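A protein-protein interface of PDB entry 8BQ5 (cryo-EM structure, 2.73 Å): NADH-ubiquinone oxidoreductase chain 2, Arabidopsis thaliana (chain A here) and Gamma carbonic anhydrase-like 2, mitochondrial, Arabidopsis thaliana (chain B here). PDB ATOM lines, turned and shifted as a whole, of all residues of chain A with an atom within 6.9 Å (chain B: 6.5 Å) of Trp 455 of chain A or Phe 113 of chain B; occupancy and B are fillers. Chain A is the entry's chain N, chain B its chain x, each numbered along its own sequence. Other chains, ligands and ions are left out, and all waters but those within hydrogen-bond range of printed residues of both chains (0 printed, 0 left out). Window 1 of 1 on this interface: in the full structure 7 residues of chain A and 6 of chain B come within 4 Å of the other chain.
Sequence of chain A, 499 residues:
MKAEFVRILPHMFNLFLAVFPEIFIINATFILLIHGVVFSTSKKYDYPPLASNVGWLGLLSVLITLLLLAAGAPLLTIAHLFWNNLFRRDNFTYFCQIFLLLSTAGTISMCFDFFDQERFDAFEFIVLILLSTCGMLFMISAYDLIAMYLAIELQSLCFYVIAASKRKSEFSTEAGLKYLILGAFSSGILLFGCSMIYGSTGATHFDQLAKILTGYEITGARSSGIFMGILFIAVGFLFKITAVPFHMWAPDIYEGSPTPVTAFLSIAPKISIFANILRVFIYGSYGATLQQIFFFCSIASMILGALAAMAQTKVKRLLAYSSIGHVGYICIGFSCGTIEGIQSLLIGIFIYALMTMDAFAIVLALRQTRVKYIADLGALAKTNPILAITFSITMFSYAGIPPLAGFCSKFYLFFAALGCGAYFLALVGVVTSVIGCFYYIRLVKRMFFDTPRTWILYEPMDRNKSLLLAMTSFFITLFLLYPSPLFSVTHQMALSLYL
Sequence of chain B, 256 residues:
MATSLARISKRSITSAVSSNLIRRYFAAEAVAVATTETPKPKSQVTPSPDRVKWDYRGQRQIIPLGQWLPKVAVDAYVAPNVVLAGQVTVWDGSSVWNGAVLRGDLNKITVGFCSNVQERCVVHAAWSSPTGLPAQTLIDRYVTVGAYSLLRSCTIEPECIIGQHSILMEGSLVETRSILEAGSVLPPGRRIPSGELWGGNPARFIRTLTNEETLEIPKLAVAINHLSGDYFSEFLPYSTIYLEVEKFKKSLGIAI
Printed residues of chain B within 4 Å of Pro 452 of chain A: Arg 141 (3.4 Å). Of chain A, only Lys 382, Thr 383 and Trp 455 come within 4 Å of Phe 113 of chain B. Printed residues of chain A within 4 Å of Tyr 142 of chain B: Trp 455 (3.9 Å). The nearest residue of chain A that does not touch Phe 113 of chain B is Leu 457 of chain A (4.1 Å).
Of the 16 printed residues of chain A, 6 touch a printed residue of chain B. Of the 16 printed residues of chain B, 4 touch a printed residue of chain A. Hydrophobic or aromatic side chains of chain B within 4 Å of the printed part of chain A: Trp 91, Phe 113 and Tyr 142. Among the printed residues, no Asp or Glu carboxylate lies within 4 Å of a Lys or Arg side-chain nitrogen of the other chain.
O of Pro 452 of chain A sits at hydrogen-bond distance from NH2 of Arg 141 of chain B (3.4 Å). O of Arg 453 of chain A is in hydrogen-bond range of NH2 of Arg 141 of chain B, at 3.1 Å. The guanidinium group of Arg 141 of chain B sits close to the indole nitrogen of Trp 455 of chain A (3.5 Å).
O of Pro 452 of chain A is in hydrogen-bond range of NE1 of Trp 455 of chain A, at 3.2 Å. O of Val 111 of chain B sits at hydrogen-bond distance from N of Trp 91 of chain B, 3.0 Å away. O of Ala 379 of chain A lies close to OG1 of Thr 383 of chain A, at 3.4 Å. The backbone NH of Tyr 142 of chain B sits at hydrogen-bond distance from the backbone carbonyl oxygen of Phe 113 of chain B, 3.0 Å away. The backbone carbonyl oxygen (O) of Trp 91 of chain B sits at hydrogen-bond distance from the side-chain hydroxyl (OG) of Ser 94 of chain B, at 2.6 Å. The backbone NH of Tyr 142 of chain B is in hydrogen-bond range of the side-chain hydroxyl of Ser 115 of chain B (3.3 Å).
CZ of Phe 113 of chain B touches O of Lys 382 of chain A (3.5 Å). Thr 383 of chain A touches Phe 113 of chain B. Phe 113 of chain B touches Trp 455 of chain A (CD2 to CZ3, 3.6 Å). Trp 455 of chain A touches Tyr 142 of chain B (CH2 to CE2, 3.9 Å). CD2 of Trp 91 of chain B touches CD1 of Leu 457 of chain A (3.5 Å).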
ATOM      1  N   ASP A 376     -11.641  17.574  22.977  1.00  0.00           N
ATOM      2  CA  ASP A 376     -12.255  18.836  22.581  1.00  0.00           C
ATOM      3  C   ASP A 376     -13.765  18.826  22.778  1.00  0.00           C
ATOM      4  O   ASP A 376     -14.389  19.892  22.764  1.00  0.00           O
ATOM      5  CB  ASP A 376     -11.930  19.148  21.119  1.00  0.00           C
ATOM      6  CG  ASP A 376     -10.457  19.422  20.891  1.00  0.00           C
ATOM      7  OD1 ASP A 376      -9.746  19.743  21.866  1.00  0.00           O
ATOM      8  OD2 ASP A 376     -10.010  19.319  19.729  1.00  0.00           O
ATOM      9  N   GLY A 378     -15.261  18.176  25.484  1.00  0.00           N
ATOM     10  CA  GLY A 378     -15.582  18.355  26.889  1.00  0.00           C
ATOM     11  C   GLY A 378     -16.655  19.411  27.091  1.00  0.00           C
ATOM     12  O   GLY A 378     -16.677  20.442  26.415  1.00  0.00           O
ATOM     13  N   ALA A 379     -17.561  19.133  28.030  1.00  0.00           N
ATOM     14  CA  ALA A 379     -18.668  20.016  28.398  1.00  0.00           C
ATOM     15  C   ALA A 379     -19.607  20.311  27.232  1.00  0.00           C
ATOM     16  O   ALA A 379     -20.284  21.342  27.229  1.00  0.00           O
ATOM     17  CB  ALA A 379     -18.157  21.329  29.003  1.00  0.00           C
ATOM     18  N   LEU A 380     -19.673  19.423  26.236  1.00  0.00           N
ATOM     19  CA  LEU A 380     -20.603  19.635  25.130  1.00  0.00           C
ATOM     20  C   LEU A 380     -22.047  19.440  25.570  1.00  0.00           C
ATOM     21  O   LEU A 380     -22.958  20.048  24.998  1.00  0.00           O
ATOM     22  CB  LEU A 380     -20.267  18.700  23.967  1.00  0.00           C
ATOM     23  CG  LEU A 380     -20.967  18.950  22.629  1.00  0.00           C
ATOM     24  CD1 LEU A 380     -20.833  20.406  22.213  1.00  0.00           C
ATOM     25  CD2 LEU A 380     -20.407  18.033  21.553  1.00  0.00           C
ATOM     26  N   LYS A 382     -23.247  20.636  28.115  1.00  0.00           N
ATOM     27  CA  LYS A 382     -23.649  21.918  28.677  1.00  0.00           C
ATOM     28  C   LYS A 382     -23.788  22.993  27.609  1.00  0.00           C
ATOM     29  O   LYS A 382     -24.756  23.761  27.622  1.00  0.00           O
ATOM     30  CB  LYS A 382     -22.633  22.369  29.730  1.00  0.00           C
ATOM     31  CG  LYS A 382     -22.295  21.317  30.779  1.00  0.00           C
ATOM     32  CD  LYS A 382     -22.913  21.599  32.143  1.00  0.00           C
ATOM     33  CE  LYS A 382     -24.376  21.988  32.069  1.00  0.00           C
ATOM     34  NZ  LYS A 382     -24.917  22.320  33.414  1.00  0.00           N
ATOM     35  N   THR A 383     -22.834  23.061  26.680  1.00  0.00           N
ATOM     36  CA  THR A 383     -22.802  24.140  25.701  1.00  0.00           C
ATOM     37  C   THR A 383     -23.733  23.899  24.522  1.00  0.00           C
ATOM     38  O   THR A 383     -24.053  24.851  23.804  1.00  0.00           O
ATOM     39  CB  THR A 383     -21.374  24.340  25.193  1.00  0.00           C
ATOM     40  OG1 THR A 383     -20.963  23.189  24.447  1.00  0.00           O
ATOM     41  CG2 THR A 383     -20.431  24.519  26.365  1.00  0.00           C
ATOM     42  N   ASN A 384     -24.166  22.660  24.303  1.00  0.00           N
ATOM     43  CA  ASN A 384     -25.144  22.326  23.275  1.00  0.00           C
ATOM     44  C   ASN A 384     -25.788  20.995  23.641  1.00  0.00           C
ATOM     45  O   ASN A 384     -25.383  19.944  23.127  1.00  0.00           O
ATOM     46  CB  ASN A 384     -24.496  22.264  21.891  1.00  0.00           C
ATOM     47  CG  ASN A 384     -25.513  22.341  20.765  1.00  0.00           C
ATOM     48  OD1 ASN A 384     -26.710  22.154  20.977  1.00  0.00           O
ATOM     49  ND2 ASN A 384     -25.038  22.633  19.562  1.00  0.00           N
ATOM     50  N   ASP A 450     -17.143  14.719  32.220  1.00  0.00           N
ATOM     51  CA  ASP A 450     -15.939  15.471  32.534  1.00  0.00           C
ATOM     52  C   ASP A 450     -16.261  16.932  32.822  1.00  0.00           C
ATOM     53  O   ASP A 450     -17.254  17.484  32.339  1.00  0.00           O
ATOM     54  CB  ASP A 450     -14.932  15.373  31.390  1.00  0.00           C
ATOM     55  CG  ASP A 450     -14.102  14.110  31.456  1.00  0.00           C
ATOM     56  OD1 ASP A 450     -13.790  13.662  32.580  1.00  0.00           O
ATOM     57  OD2 ASP A 450     -13.767  13.560  30.388  1.00  0.00           O
ATOM     58  N   THR A 451     -15.405  17.555  33.629  1.00  0.00           N
ATOM     59  CA  THR A 451     -15.531  18.963  34.004  1.00  0.00           C
ATOM     60  C   THR A 451     -14.190  19.635  33.745  1.00  0.00           C
ATOM     61  O   THR A 451     -13.417  19.891  34.678  1.00  0.00           O
ATOM     62  CB  THR A 451     -15.961  19.116  35.464  1.00  0.00           C
ATOM     63  OG1 THR A 451     -15.122  18.314  36.303  1.00  0.00           O
ATOM     64  CG2 THR A 451     -17.406  18.686  35.643  1.00  0.00           C
ATOM     65  N   PRO A 452     -13.881  19.932  32.485  1.00  0.00           N
ATOM     66  CA  PRO A 452     -12.569  20.501  32.160  1.00  0.00           C
ATOM     67  C   PRO A 452     -12.437  21.938  32.639  1.00  0.00           C
ATOM     68  O   PRO A 452     -13.416  22.667  32.806  1.00  0.00           O
ATOM     69  CB  PRO A 452     -12.505  20.423  30.630  1.00  0.00           C
ATOM     70  CG  PRO A 452     -13.882  20.070  30.163  1.00  0.00           C
ATOM     71  CD  PRO A 452     -14.797  19.936  31.336  1.00  0.00           C
ATOM     72  N   ARG A 453     -11.185  22.340  32.863  1.00  0.00           N
ATOM     73  CA  ARG A 453     -10.905  23.723  33.233  1.00  0.00           C
ATOM     74  C   ARG A 453     -11.198  24.678  32.082  1.00  0.00           C
ATOM     75  O   ARG A 453     -11.734  25.770  32.296  1.00  0.00           O
ATOM     76  CB  ARG A 453      -9.456  23.859  33.696  1.00  0.00           C
ATOM     77  CG  ARG A 453      -8.998  25.293  33.911  1.00  0.00           C
ATOM     78  CD  ARG A 453      -9.612  25.904  35.165  1.00  0.00           C
ATOM     79  NE  ARG A 453      -9.404  27.345  35.290  1.00  0.00           N
ATOM     80  CZ  ARG A 453      -9.672  28.257  34.361  1.00  0.00           C
ATOM     81  NH1 ARG A 453     -10.259  27.939  33.218  1.00  0.00           N
ATOM     82  NH2 ARG A 453      -9.364  29.529  34.596  1.00  0.00           N
ATOM     83  N   THR A 454     -10.861  24.286  30.858  1.00  0.00           N
ATOM     84  CA  THR A 454     -11.078  25.113  29.681  1.00  0.00           C
ATOM     85  C   THR A 454     -12.086  24.435  28.765  1.00  0.00           C
ATOM     86  O   THR A 454     -11.960  23.243  28.468  1.00  0.00           O
ATOM     87  CB  THR A 454      -9.764  25.362  28.937  1.00  0.00           C
ATOM     88  OG1 THR A 454      -8.909  26.182  29.744  1.00  0.00           O
ATOM     89  CG2 THR A 454     -10.025  26.069  27.621  1.00  0.00           C
ATOM     90  N   TRP A 455     -13.087  25.192  28.328  1.00  0.00           N
ATOM     91  CA  TRP A 455     -14.115  24.694  27.429  1.00  0.00           C
ATOM     92  C   TRP A 455     -13.854  25.184  26.011  1.00  0.00           C
ATOM     93  O   TRP A 455     -13.106  26.139  25.791  1.00  0.00           O
ATOM     94  CB  TRP A 455     -15.508  25.148  27.872  1.00  0.00           C
ATOM     95  CG  TRP A 455     -15.973  24.599  29.190  1.00  0.00           C
ATOM     96  CD1 TRP A 455     -15.225  23.941  30.121  1.00  0.00           C
ATOM     97  CD2 TRP A 455     -17.299  24.679  29.725  1.00  0.00           C
ATOM     98  NE1 TRP A 455     -16.003  23.600  31.199  1.00  0.00           N
ATOM     99  CE2 TRP A 455     -17.281  24.045  30.981  1.00  0.00           C
ATOM    100  CE3 TRP A 455     -18.498  25.227  29.263  1.00  0.00           C
ATOM    101  CZ2 TRP A 455     -18.417  23.939  31.779  1.00  0.00           C
ATOM    102  CZ3 TRP A 455     -19.623  25.121  30.056  1.00  0.00           C
ATOM    103  CH2 TRP A 455     -19.576  24.483  31.300  1.00  0.00           C
ATOM    104  N   ILE A 456     -14.477  24.515  25.048  1.00  0.00           N
ATOM    105  CA  ILE A 456     -14.491  24.958  23.660  1.00  0.00           C
ATOM    106  C   ILE A 456     -15.945  25.154  23.258  1.00  0.00           C
ATOM    107  O   ILE A 456     -16.748  24.217  23.330  1.00  0.00           O
ATOM    108  CB  ILE A 456     -13.783  23.961  22.733  1.00  0.00           C
ATOM    109  CG1 ILE A 456     -12.271  24.027  22.941  1.00  0.00           C
ATOM    110  CG2 ILE A 456     -14.115  24.263  21.285  1.00  0.00           C
ATOM    111  CD1 ILE A 456     -11.555  22.753  22.582  1.00  0.00           C
ATOM    112  N   LEU A 457     -16.282  26.372  22.847  1.00  0.00           N
ATOM    113  CA  LEU A 457     -17.641  26.710  22.445  1.00  0.00           C
ATOM    114  C   LEU A 457     -17.741  26.622  20.928  1.00  0.00           C
ATOM    115  O   LEU A 457     -17.032  27.337  20.212  1.00  0.00           O
ATOM    116  CB  LEU A 457     -18.016  28.109  22.933  1.00  0.00           C
ATOM    117  CG  LEU A 457     -17.705  28.416  24.400  1.00  0.00           C
ATOM    118  CD1 LEU A 457     -18.163  29.817  24.769  1.00  0.00           C
ATOM    119  CD2 LEU A 457     -18.346  27.387  25.312  1.00  0.00           C
ATOM    120  N   TYR A 458     -18.631  25.764  20.445  1.00  0.00           N
ATOM    121  CA  TYR A 458     -18.722  25.439  19.029  1.00  0.00           C
ATOM    122  C   TYR A 458     -19.783  26.287  18.339  1.00  0.00           C
ATOM    123  O   TYR A 458     -20.856  26.536  18.896  1.00  0.00           O
ATOM    124  CB  TYR A 458     -19.033  23.953  18.846  1.00  0.00           C
ATOM    125  CG  TYR A 458     -17.878  23.065  19.235  1.00  0.00           C
ATOM    126  CD1 TYR A 458     -16.893  22.737  18.317  1.00  0.00           C
ATOM    127  CD2 TYR A 458     -17.755  22.579  20.528  1.00  0.00           C
ATOM    128  CE1 TYR A 458     -15.828  21.938  18.668  1.00  0.00           C
ATOM    129  CE2 TYR A 458     -16.693  21.779  20.889  1.00  0.00           C
ATOM    130  CZ  TYR A 458     -15.733  21.461  19.954  1.00  0.00           C
ATOM    131  OH  TYR A 458     -14.672  20.664  20.305  1.00  0.00           O
ATOM    132  N   ASP B  75     -28.181  32.548  20.581  1.00  0.00           N
ATOM    133  CA  ASP B  75     -28.989  32.323  21.773  1.00  0.00           C
ATOM    134  C   ASP B  75     -28.549  33.193  22.951  1.00  0.00           C
ATOM    135  O   ASP B  75     -28.666  32.792  24.110  1.00  0.00           O
ATOM    136  CB  ASP B  75     -28.991  30.838  22.145  1.00  0.00           C
ATOM    137  CG  ASP B  75     -27.730  30.402  22.874  1.00  0.00           C
ATOM    138  OD1 ASP B  75     -26.730  31.144  22.848  1.00  0.00           O
ATOM    139  OD2 ASP B  75     -27.747  29.320  23.494  1.00  0.00           O
ATOM    140  N   TRP B  91     -20.991  35.333  23.987  1.00  0.00           N
ATOM    141  CA  TRP B  91     -21.088  33.904  23.731  1.00  0.00           C
ATOM    142  C   TRP B  91     -22.466  33.355  24.091  1.00  0.00           C
ATOM    143  O   TRP B  91     -23.374  34.079  24.504  1.00  0.00           O
ATOM    144  CB  TRP B  91     -20.003  33.148  24.495  1.00  0.00           C
ATOM    145  CG  TRP B  91     -18.670  33.200  23.835  1.00  0.00           C
ATOM    146  CD1 TRP B  91     -17.577  33.894  24.257  1.00  0.00           C
ATOM    147  CD2 TRP B  91     -18.290  32.551  22.618  1.00  0.00           C
ATOM    148  NE1 TRP B  91     -16.533  33.704  23.387  1.00  0.00           N
ATOM    149  CE2 TRP B  91     -16.946  32.885  22.370  1.00  0.00           C
ATOM    150  CE3 TRP B  91     -18.955  31.714  21.717  1.00  0.00           C
ATOM    151  CZ2 TRP B  91     -16.254  32.414  21.259  1.00  0.00           C
ATOM    152  CZ3 TRP B  91     -18.266  31.247  20.616  1.00  0.00           C
ATOM    153  CH2 TRP B  91     -16.929  31.597  20.396  1.00  0.00           C
ATOM    154  N   ASP B  92     -22.608  32.040  23.942  1.00  0.00           N
ATOM    155  CA  ASP B  92     -23.899  31.385  24.090  1.00  0.00           C
ATOM    156  C   ASP B  92     -24.399  31.459  25.527  1.00  0.00           C
ATOM    157  O   ASP B  92     -23.649  31.229  26.478  1.00  0.00           O
ATOM    158  CB  ASP B  92     -23.796  29.927  23.647  1.00  0.00           C
ATOM    159  CG  ASP B  92     -23.375  29.790  22.200  1.00  0.00           C
ATOM    160  OD1 ASP B  92     -24.133  29.187  21.413  1.00  0.00           O
ATOM    161  OD2 ASP B  92     -22.288  30.297  21.847  1.00  0.00           O
ATOM    162  N   GLY B  93     -25.682  31.779  25.678  1.00  0.00           N
ATOM    163  CA  GLY B  93     -26.304  31.835  26.981  1.00  0.00           C
ATOM    164  C   GLY B  93     -25.972  33.063  27.795  1.00  0.00           C
ATOM    165  O   GLY B  93     -26.407  33.156  28.948  1.00  0.00           O
ATOM    166  N   SER B  94     -25.220  34.004  27.239  1.00  0.00           N
ATOM    167  CA  SER B  94     -24.852  35.210  27.954  1.00  0.00           C
ATOM    168  C   SER B  94     -25.884  36.310  27.711  1.00  0.00           C
ATOM    169  O   SER B  94     -26.636  36.290  26.735  1.00  0.00           O
ATOM    170  CB  SER B  94     -23.457  35.666  27.537  1.00  0.00           C
ATOM    171  OG  SER B  94     -23.441  36.065  26.184  1.00  0.00           O
ATOM    172  N   VAL B 111     -17.473  38.013  26.566  1.00  0.00           N
ATOM    173  CA  VAL B 111     -18.406  37.609  27.612  1.00  0.00           C
ATOM    174  C   VAL B 111     -18.662  36.118  27.445  1.00  0.00           C
ATOM    175  O   VAL B 111     -19.290  35.693  26.468  1.00  0.00           O
ATOM    176  CB  VAL B 111     -19.715  38.411  27.552  1.00  0.00           C
ATOM    177  CG1 VAL B 111     -20.620  38.035  28.717  1.00  0.00           C
ATOM    178  CG2 VAL B 111     -19.423  39.902  27.557  1.00  0.00           C
ATOM    179  N   GLY B 112     -18.196  35.329  28.412  1.00  0.00           N
ATOM    180  CA  GLY B 112     -18.156  33.891  28.275  1.00  0.00           C
ATOM    181  C   GLY B 112     -19.507  33.219  28.419  1.00  0.00           C
ATOM    182  O   GLY B 112     -20.550  33.852  28.580  1.00  0.00           O
ATOM    183  N   PHE B 113     -19.466  31.889  28.362  1.00  0.00           N
ATOM    184  CA  PHE B 113     -20.676  31.077  28.376  1.00  0.00           C
ATOM    185  C   PHE B 113     -21.504  31.340  29.628  1.00  0.00           C
ATOM    186  O   PHE B 113     -21.003  31.247  30.750  1.00  0.00           O
ATOM    187  CB  PHE B 113     -20.296  29.597  28.289  1.00  0.00           C
ATOM    188  CG  PHE B 113     -21.455  28.658  28.443  1.00  0.00           C
ATOM    189  CD1 PHE B 113     -22.301  28.402  27.378  1.00  0.00           C
ATOM    190  CD2 PHE B 113     -21.695  28.025  29.651  1.00  0.00           C
ATOM    191  CE1 PHE B 113     -23.365  27.537  27.516  1.00  0.00           C
ATOM    192  CE2 PHE B 113     -22.759  27.159  29.794  1.00  0.00           C
ATOM    193  CZ  PHE B 113     -23.594  26.915  28.726  1.00  0.00           C
ATOM    194  N   CYS B 114     -22.777  31.679  29.424  1.00  0.00           N
ATOM    195  CA  CYS B 114     -23.749  31.838  30.509  1.00  0.00           C
ATOM    196  C   CYS B 114     -23.356  32.943  31.491  1.00  0.00           C
ATOM    197  O   CYS B 114     -23.791  32.942  32.644  1.00  0.00           O
ATOM    198  CB  CYS B 114     -23.962  30.516  31.253  1.00  0.00           C
ATOM    199  SG  CYS B 114     -25.204  30.575  32.559  1.00  0.00           S
ATOM    200  N   SER B 115     -22.539  33.895  31.054  1.00  0.00           N
ATOM    201  CA  SER B 115     -22.166  35.044  31.867  1.00  0.00           C
ATOM    202  C   SER B 115     -23.110  36.208  31.585  1.00  0.00           C
ATOM    203  O   SER B 115     -23.719  36.294  30.521  1.00  0.00           O
ATOM    204  CB  SER B 115     -20.719  35.460  31.588  1.00  0.00           C
ATOM    205  OG  SER B 115     -19.807  34.577  32.213  1.00  0.00           O
ATOM    206  N   ILE B 139     -14.232  38.007  30.405  1.00  0.00           N
ATOM    207  CA  ILE B 139     -15.248  37.568  31.352  1.00  0.00           C
ATOM    208  C   ILE B 139     -15.540  36.108  31.034  1.00  0.00           C
ATOM    209  O   ILE B 139     -16.149  35.797  30.007  1.00  0.00           O
ATOM    210  CB  ILE B 139     -16.513  38.432  31.266  1.00  0.00           C
ATOM    211  CG1 ILE B 139     -16.186  39.887  31.608  1.00  0.00           C
ATOM    212  CG2 ILE B 139     -17.593  37.900  32.188  1.00  0.00           C
ATOM    213  CD1 ILE B 139     -17.058  40.889  30.895  1.00  0.00           C
ATOM    214  N   ASP B 140     -15.100  35.205  31.907  1.00  0.00           N
ATOM    215  CA  ASP B 140     -15.212  33.776  31.644  1.00  0.00           C
ATOM    216  C   ASP B 140     -16.637  33.308  31.935  1.00  0.00           C
ATOM    217  O   ASP B 140     -17.557  34.108  32.125  1.00  0.00           O
ATOM    218  CB  ASP B 140     -14.170  33.004  32.451  1.00  0.00           C
ATOM    219  CG  ASP B 140     -13.561  31.848  31.668  1.00  0.00           C
ATOM    220  OD1 ASP B 140     -12.405  31.473  31.956  1.00  0.00           O
ATOM    221  OD2 ASP B 140     -14.236  31.312  30.764  1.00  0.00           O
ATOM    222  N   ARG B 141     -16.835  31.995  31.965  1.00  0.00           N
ATOM    223  CA  ARG B 141     -18.169  31.430  32.094  1.00  0.00           C
ATOM    224  C   ARG B 141     -18.705  31.563  33.517  1.00  0.00           C
ATOM    225  O   ARG B 141     -17.949  31.656  34.486  1.00  0.00           O
ATOM    226  CB  ARG B 141     -18.163  29.959  31.685  1.00  0.00           C
ATOM    227  CG  ARG B 141     -17.252  29.096  32.529  1.00  0.00           C
ATOM    228  CD  ARG B 141     -17.428  27.629  32.203  1.00  0.00           C
ATOM    229  NE  ARG B 141     -16.557  26.792  33.016  1.00  0.00           N
ATOM    230  CZ  ARG B 141     -15.283  26.551  32.738  1.00  0.00           C
ATOM    231  NH1 ARG B 141     -14.695  27.079  31.678  1.00  0.00           N
ATOM    232  NH2 ARG B 141     -14.581  25.763  33.547  1.00  0.00           N
ATOM    233  N   TYR B 142     -20.036  31.569  33.623  1.00  0.00           N
ATOM    234  CA  TYR B 142     -20.744  31.591  34.904  1.00  0.00           C
ATOM    235  C   TYR B 142     -20.311  32.770  35.770  1.00  0.00           C
ATOM    236  O   TYR B 142     -20.181  32.660  36.990  1.00  0.00           O
ATOM    237  CB  TYR B 142     -20.565  30.272  35.658  1.00  0.00           C
ATOM    238  CG  TYR B 142     -21.190  29.085  34.969  1.00  0.00           C
ATOM    239  CD1 TYR B 142     -22.543  29.068  34.662  1.00  0.00           C
ATOM    240  CD2 TYR B 142     -20.425  27.982  34.619  1.00  0.00           C
ATOM    241  CE1 TYR B 142     -23.116  27.983  34.031  1.00  0.00           C
ATOM    242  CE2 TYR B 142     -20.989  26.895  33.988  1.00  0.00           C
ATOM    243  CZ  TYR B 142     -22.334  26.900  33.696  1.00  0.00           C
ATOM    244  OH  TYR B 142     -22.895  25.815  33.064  1.00  0.00           O
ATOM    245  N   VAL B 143     -20.094  33.915  35.135  1.00  0.00           N
ATOM    246  CA  VAL B 143     -19.686  35.130  35.825  1.00  0.00           C
ATOM    247  C   VAL B 143     -20.877  36.073  35.875  1.00  0.00           C
ATOM    248  O   VAL B 143     -21.541  36.302  34.858  1.00  0.00           O
ATOM    249  CB  VAL B 143     -18.477  35.793  35.146  1.00  0.00           C
ATOM    250  CG1 VAL B 143     -18.213  37.161  35.754  1.00  0.00           C
ATOM    251  CG2 VAL B 143     -17.255  34.909  35.287  1.00  0.00           C
ATOM    252  N   ALA B 221     -25.720  32.409  37.990  1.00  0.00           N
ATOM    253  CA  ALA B 221     -25.578  32.687  36.562  1.00  0.00           C
ATOM    254  C   ALA B 221     -26.681  32.007  35.753  1.00  0.00           C
ATOM    255  O   ALA B 221     -27.258  32.608  34.836  1.00  0.00           O
ATOM    256  CB  ALA B 221     -24.199  32.250  36.070  1.00  0.00           C
